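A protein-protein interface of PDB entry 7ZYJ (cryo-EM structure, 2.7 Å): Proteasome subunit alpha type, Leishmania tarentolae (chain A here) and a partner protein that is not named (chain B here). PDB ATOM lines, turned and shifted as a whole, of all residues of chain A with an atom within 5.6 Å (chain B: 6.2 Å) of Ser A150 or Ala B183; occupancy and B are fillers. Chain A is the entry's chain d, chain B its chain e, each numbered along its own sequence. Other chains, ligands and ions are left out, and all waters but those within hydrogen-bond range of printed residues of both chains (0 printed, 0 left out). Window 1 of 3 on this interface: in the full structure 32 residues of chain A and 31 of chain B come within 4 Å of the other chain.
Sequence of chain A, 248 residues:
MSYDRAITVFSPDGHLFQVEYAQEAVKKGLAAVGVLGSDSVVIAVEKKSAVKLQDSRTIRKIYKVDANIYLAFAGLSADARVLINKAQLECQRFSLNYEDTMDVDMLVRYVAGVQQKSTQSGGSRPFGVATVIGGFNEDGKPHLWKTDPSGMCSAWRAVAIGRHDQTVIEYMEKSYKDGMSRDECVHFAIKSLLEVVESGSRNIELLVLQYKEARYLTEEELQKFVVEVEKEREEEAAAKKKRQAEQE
The backbone carbonyl oxygen (O) of Thr A119 is in hydrogen-bond range of the guanidinium group (NE) of Arg B235 (3.0 Å).
NE2 of Gln A116 lies close to OD1 of Asp B184 (2.2 Å).
Ala B183 touches Gln A116 (O to CG, 3.5 Å).
OE1 of Gln A116 touches CG1 of Ile B187 (3.5 Å).
NE2 of Gln A116 touches NH2 of Arg B235 (3.96 Å).
Ser A150 touches Ala B183 (O to CB, 3.2 Å).
Gly A151 touches Ala B183 (O to CB, 3.6 Å).
CG of Met A152 touches CG2 of Val B182, at 3.6 Å.
Met A152 touches Ala B183.
Of the 10 printed residues of chain A, 5 touch a printed residue of chain B.
Hydrophobic or aromatic side chains of chain A that line the printed part of chain B: Met A152.
Of the 9 printed residues of chain B, 5 touch a printed residue of chain A.
Hydrophobic or aromatic side chains of chain B within 4 Å of the printed part of chain A: Val B182, Ala B183 and Ile B187.
Along chain B the printed residues that touch a printed residue of chain A span positions 182 to 235.
Of the printed residues of chain B, Thr A119 touches Arg B235.
Ser A150 touches one residue of chain B.
Of the printed residues of chain B, Met A152 touches Val B182 (3.6 Å) and Ala B183 (3.99 Å).
Met B181 touches none of the printed residues of chain A.
Of the printed residues of chain A, Val B182 touches Met A152 (3.6 Å).
Of the printed residues of chain A, Ala B183 touches Gln A116 (3.5 Å), Ser A150 (3.2 Å), Gly A151 (3.6 Å) and Met A152 (3.99 Å).
Printed residues of chain A within 4 Å of Ile B187: Gln A116 (3.5 Å).
Of the printed residues of chain A, Arg B235 touches Gln A116 (3.96 Å) and Thr A119 (3.0 Å).
The side-chain hydroxyl (OG) of Ser A150 sits at hydrogen-bond distance from the side-chain carboxylate (OD2) of Asp A148 (2.9 Å).
The backbone NH (N) of Gly A151 is in hydrogen-bond range of the side-chain carboxylate (OD1) of Asp A148, at 3.2 Å.
The guanidinium group of Arg B235 lies within salt-bridge range of the side-chain carboxylate of Asp B184 (3.2 Å).
The side-chain carboxylate (OD1) of Asp A148 is in hydrogen-bond range of the backbone NH (N) of Met A152, at 2.6 Å.
The side-chain hydroxyl (OG1) of Thr A119 sits at hydrogen-bond distance from the backbone carbonyl oxygen (O) of Gln A116 (2.6 Å).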
ATOM      1  N   VAL A  19     -27.247 -26.750 -14.837  1.00  0.00           N
ATOM      2  CA  VAL A  19     -28.483 -26.611 -14.074  1.00  0.00           C
ATOM      3  C   VAL A  19     -29.697 -26.828 -14.971  1.00  0.00           C
ATOM      4  O   VAL A  19     -30.663 -27.492 -14.578  1.00  0.00           O
ATOM      5  CB  VAL A  19     -28.526 -25.237 -13.381  1.00  0.00           C
ATOM      6  CG1 VAL A  19     -29.845 -25.052 -12.655  1.00  0.00           C
ATOM      7  CG2 VAL A  19     -27.359 -25.097 -12.419  1.00  0.00           C
ATOM      8  N   ALA A 112     -32.140 -27.102   0.039  1.00  0.00           N
ATOM      9  CA  ALA A 112     -31.901 -26.144  -1.033  1.00  0.00           C
ATOM     10  C   ALA A 112     -30.450 -25.687  -1.047  1.00  0.00           C
ATOM     11  O   ALA A 112     -29.858 -25.506  -2.116  1.00  0.00           O
ATOM     12  CB  ALA A 112     -32.842 -24.948  -0.886  1.00  0.00           C
ATOM     13  N   GLN A 115     -28.383 -28.461  -2.610  1.00  0.00           N
ATOM     14  CA  GLN A 115     -28.557 -28.448  -4.060  1.00  0.00           C
ATOM     15  C   GLN A 115     -27.805 -27.286  -4.698  1.00  0.00           C
ATOM     16  O   GLN A 115     -27.222 -27.434  -5.777  1.00  0.00           O
ATOM     17  CB  GLN A 115     -30.043 -28.389  -4.414  1.00  0.00           C
ATOM     18  CG  GLN A 115     -30.854 -29.556  -3.882  1.00  0.00           C
ATOM     19  CD  GLN A 115     -31.921 -30.019  -4.851  1.00  0.00           C
ATOM     20  OE1 GLN A 115     -31.680 -30.131  -6.052  1.00  0.00           O
ATOM     21  NE2 GLN A 115     -33.113 -30.288  -4.333  1.00  0.00           N
ATOM     22  N   GLN A 116     -27.814 -26.120  -4.049  1.00  0.00           N
ATOM     23  CA  GLN A 116     -27.072 -24.974  -4.563  1.00  0.00           C
ATOM     24  C   GLN A 116     -25.573 -25.248  -4.579  1.00  0.00           C
ATOM     25  O   GLN A 116     -24.892 -24.960  -5.570  1.00  0.00           O
ATOM     26  CB  GLN A 116     -27.388 -23.731  -3.728  1.00  0.00           C
ATOM     27  CG  GLN A 116     -26.985 -22.418  -4.379  1.00  0.00           C
ATOM     28  CD  GLN A 116     -25.513 -22.101  -4.197  1.00  0.00           C
ATOM     29  OE1 GLN A 116     -24.867 -22.602  -3.277  1.00  0.00           O
ATOM     30  NE2 GLN A 116     -24.973 -21.271  -5.077  1.00  0.00           N
ATOM     31  N   THR A 119     -24.225 -27.051  -7.418  1.00  0.00           N
ATOM     32  CA  THR A 119     -24.093 -26.297  -8.656  1.00  0.00           C
ATOM     33  C   THR A 119     -22.910 -25.338  -8.643  1.00  0.00           C
ATOM     34  O   THR A 119     -22.720 -24.594  -9.609  1.00  0.00           O
ATOM     35  CB  THR A 119     -25.379 -25.520  -8.946  1.00  0.00           C
ATOM     36  OG1 THR A 119     -25.491 -24.421  -8.034  1.00  0.00           O
ATOM     37  CG2 THR A 119     -26.591 -26.420  -8.798  1.00  0.00           C
ATOM     38  N   ASP A 148     -35.838 -26.993  -6.408  1.00  0.00           N
ATOM     39  CA  ASP A 148     -35.461 -27.298  -7.782  1.00  0.00           C
ATOM     40  C   ASP A 148     -33.967 -27.598  -7.843  1.00  0.00           C
ATOM     41  O   ASP A 148     -33.250 -27.336  -6.869  1.00  0.00           O
ATOM     42  CB  ASP A 148     -35.844 -26.137  -8.705  1.00  0.00           C
ATOM     43  CG  ASP A 148     -35.301 -24.806  -8.233  1.00  0.00           C
ATOM     44  OD1 ASP A 148     -34.500 -24.786  -7.277  1.00  0.00           O
ATOM     45  OD2 ASP A 148     -35.675 -23.772  -8.824  1.00  0.00           O
ATOM     46  N   PRO A 149     -33.458 -28.157  -8.947  1.00  0.00           N
ATOM     47  CA  PRO A 149     -32.018 -28.459  -9.016  1.00  0.00           C
ATOM     48  C   PRO A 149     -31.121 -27.249  -8.823  1.00  0.00           C
ATOM     49  O   PRO A 149     -29.977 -27.413  -8.382  1.00  0.00           O
ATOM     50  CB  PRO A 149     -31.853 -29.053 -10.420  1.00  0.00           C
ATOM     51  CG  PRO A 149     -33.173 -29.643 -10.723  1.00  0.00           C
ATOM     52  CD  PRO A 149     -34.192 -28.749 -10.080  1.00  0.00           C
ATOM     53  N   SER A 150     -31.594 -26.043  -9.136  1.00  0.00           N
ATOM     54  CA  SER A 150     -30.790 -24.842  -8.946  1.00  0.00           C
ATOM     55  C   SER A 150     -30.620 -24.463  -7.482  1.00  0.00           C
ATOM     56  O   SER A 150     -29.792 -23.599  -7.178  1.00  0.00           O
ATOM     57  CB  SER A 150     -31.411 -23.667  -9.705  1.00  0.00           C
ATOM     58  OG  SER A 150     -32.798 -23.564  -9.440  1.00  0.00           O
ATOM     59  N   GLY A 151     -31.364 -25.084  -6.576  1.00  0.00           N
ATOM     60  CA  GLY A 151     -31.291 -24.757  -5.170  1.00  0.00           C
ATOM     61  C   GLY A 151     -32.274 -23.713  -4.691  1.00  0.00           C
ATOM     62  O   GLY A 151     -32.097 -23.188  -3.586  1.00  0.00           O
ATOM     63  N   MET A 152     -33.293 -23.391  -5.481  1.00  0.00           N
ATOM     64  CA  MET A 152     -34.305 -22.417  -5.095  1.00  0.00           C
ATOM     65  C   MET A 152     -35.434 -23.129  -4.359  1.00  0.00           C
ATOM     66  O   MET A 152     -35.969 -24.129  -4.850  1.00  0.00           O
ATOM     67  CB  MET A 152     -34.840 -21.681  -6.322  1.00  0.00           C
ATOM     68  CG  MET A 152     -35.864 -20.609  -6.005  1.00  0.00           C
ATOM     69  SD  MET A 152     -36.448 -19.750  -7.476  1.00  0.00           S
ATOM     70  CE  MET A 152     -37.457 -21.020  -8.235  1.00  0.00           C
ATOM     71  N   MET B 181     -29.927 -14.811  -9.482  1.00  0.00           N
ATOM     72  CA  MET B 181     -30.135 -16.173  -9.006  1.00  0.00           C
ATOM     73  C   MET B 181     -30.313 -16.154  -7.493  1.00  0.00           C
ATOM     74  O   MET B 181     -29.337 -16.012  -6.751  1.00  0.00           O
ATOM     75  CB  MET B 181     -28.958 -17.062  -9.403  1.00  0.00           C
ATOM     76  CG  MET B 181     -28.841 -17.290 -10.899  1.00  0.00           C
ATOM     77  SD  MET B 181     -27.443 -18.332 -11.349  1.00  0.00           S
ATOM     78  CE  MET B 181     -27.568 -18.295 -13.134  1.00  0.00           C
ATOM     79  N   VAL B 182     -31.559 -16.311  -7.039  1.00  0.00           N
ATOM     80  CA  VAL B 182     -31.848 -16.223  -5.612  1.00  0.00           C
ATOM     81  C   VAL B 182     -31.160 -17.323  -4.815  1.00  0.00           C
ATOM     82  O   VAL B 182     -30.859 -17.125  -3.633  1.00  0.00           O
ATOM     83  CB  VAL B 182     -33.369 -16.245  -5.372  1.00  0.00           C
ATOM     84  CG1 VAL B 182     -34.024 -15.053  -6.046  1.00  0.00           C
ATOM     85  CG2 VAL B 182     -33.969 -17.540  -5.887  1.00  0.00           C
ATOM     86  N   ALA B 183     -30.908 -18.483  -5.425  1.00  0.00           N
ATOM     87  CA  ALA B 183     -30.241 -19.563  -4.707  1.00  0.00           C
ATOM     88  C   ALA B 183     -28.821 -19.182  -4.306  1.00  0.00           C
ATOM     89  O   ALA B 183     -28.394 -19.485  -3.186  1.00  0.00           O
ATOM     90  CB  ALA B 183     -30.230 -20.832  -5.557  1.00  0.00           C
ATOM     91  N   ASP B 184     -28.079 -18.526  -5.199  1.00  0.00           N
ATOM     92  CA  ASP B 184     -26.736 -18.068  -4.866  1.00  0.00           C
ATOM     93  C   ASP B 184     -26.745 -16.881  -3.915  1.00  0.00           C
ATOM     94  O   ASP B 184     -25.786 -16.702  -3.159  1.00  0.00           O
ATOM     95  CB  ASP B 184     -25.971 -17.694  -6.138  1.00  0.00           C
ATOM     96  CG  ASP B 184     -25.887 -18.833  -7.131  1.00  0.00           C
ATOM     97  OD1 ASP B 184     -25.879 -20.004  -6.700  1.00  0.00           O
ATOM     98  OD2 ASP B 184     -25.821 -18.556  -8.346  1.00  0.00           O
ATOM     99  N   ALA B 185     -27.802 -16.064  -3.943  1.00  0.00           N
ATOM    100  CA  ALA B 185     -27.869 -14.902  -3.065  1.00  0.00           C
ATOM    101  C   ALA B 185     -27.975 -15.303  -1.600  1.00  0.00           C
ATOM    102  O   ALA B 185     -27.544 -14.551  -0.718  1.00  0.00           O
ATOM    103  CB  ALA B 185     -29.050 -14.018  -3.457  1.00  0.00           C
ATOM    104  N   ARG B 186     -28.554 -16.474  -1.321  1.00  0.00           N
ATOM    105  CA  ARG B 186     -28.662 -16.934   0.058  1.00  0.00           C
ATOM    106  C   ARG B 186     -27.287 -17.117   0.686  1.00  0.00           C
ATOM    107  O   ARG B 186     -27.087 -16.787   1.859  1.00  0.00           O
ATOM    108  CB  ARG B 186     -29.456 -18.239   0.119  1.00  0.00           C
ATOM    109  CG  ARG B 186     -30.791 -18.194  -0.598  1.00  0.00           C
ATOM    110  CD  ARG B 186     -31.837 -17.472   0.229  1.00  0.00           C
ATOM    111  NE  ARG B 186     -33.187 -17.729  -0.258  1.00  0.00           N
ATOM    112  CZ  ARG B 186     -34.023 -16.790  -0.679  1.00  0.00           C
ATOM    113  NH1 ARG B 186     -33.680 -15.512  -0.684  1.00  0.00           N
ATOM    114  NH2 ARG B 186     -35.232 -17.141  -1.105  1.00  0.00           N
ATOM    115  N   ILE B 187     -26.330 -17.641  -0.081  1.00  0.00           N
ATOM    116  CA  ILE B 187     -24.972 -17.813   0.429  1.00  0.00           C
ATOM    117  C   ILE B 187     -24.364 -16.465   0.794  1.00  0.00           C
ATOM    118  O   ILE B 187     -23.759 -16.307   1.863  1.00  0.00           O
ATOM    119  CB  ILE B 187     -24.109 -18.563  -0.603  1.00  0.00           C
ATOM    120  CG1 ILE B 187     -24.800 -19.854  -1.042  1.00  0.00           C
ATOM    121  CG2 ILE B 187     -22.731 -18.858  -0.033  1.00  0.00           C
ATOM    122  CD1 ILE B 187     -25.002 -20.849   0.076  1.00  0.00           C
ATOM    123  N   ARG B 235     -17.436 -21.233 -10.223  1.00  0.00           N
ATOM    124  CA  ARG B 235     -17.976 -20.151 -11.033  1.00  0.00           C
ATOM    125  C   ARG B 235     -18.271 -18.971 -10.120  1.00  0.00           C
ATOM    126  O   ARG B 235     -18.427 -19.146  -8.907  1.00  0.00           O
ATOM    127  CB  ARG B 235     -19.252 -20.594 -11.766  1.00  0.00           C
ATOM    128  CG  ARG B 235     -20.290 -21.211 -10.849  1.00  0.00           C
ATOM    129  CD  ARG B 235     -21.651 -21.286 -11.514  1.00  0.00           C
ATOM    130  NE  ARG B 235     -22.669 -21.789 -10.601  1.00  0.00           N
ATOM    131  CZ  ARG B 235     -23.353 -21.033  -9.753  1.00  0.00           C
ATOM    132  NH1 ARG B 235     -23.155 -19.728  -9.676  1.00  0.00           N
ATOM    133  NH2 ARG B 235     -24.256 -21.602  -8.960  1.00  0.00           N
ATOM    134  N   VAL B 239     -25.285 -13.222  -8.915  1.00  0.00           N
ATOM    135  CA  VAL B 239     -26.078 -12.356  -8.057  1.00  0.00           C
ATOM    136  C   VAL B 239     -25.460 -10.968  -8.031  1.00  0.00           C
ATOM    137  O   VAL B 239     -24.238 -10.810  -7.935  1.00  0.00           O
ATOM    138  CB  VAL B 239     -26.185 -12.915  -6.620  1.00  0.00           C
ATOM    139  CG1 VAL B 239     -27.030 -11.999  -5.748  1.00  0.00           C
ATOM    140  CG2 VAL B 239     -26.757 -14.306  -6.639  1.00  0.00           C
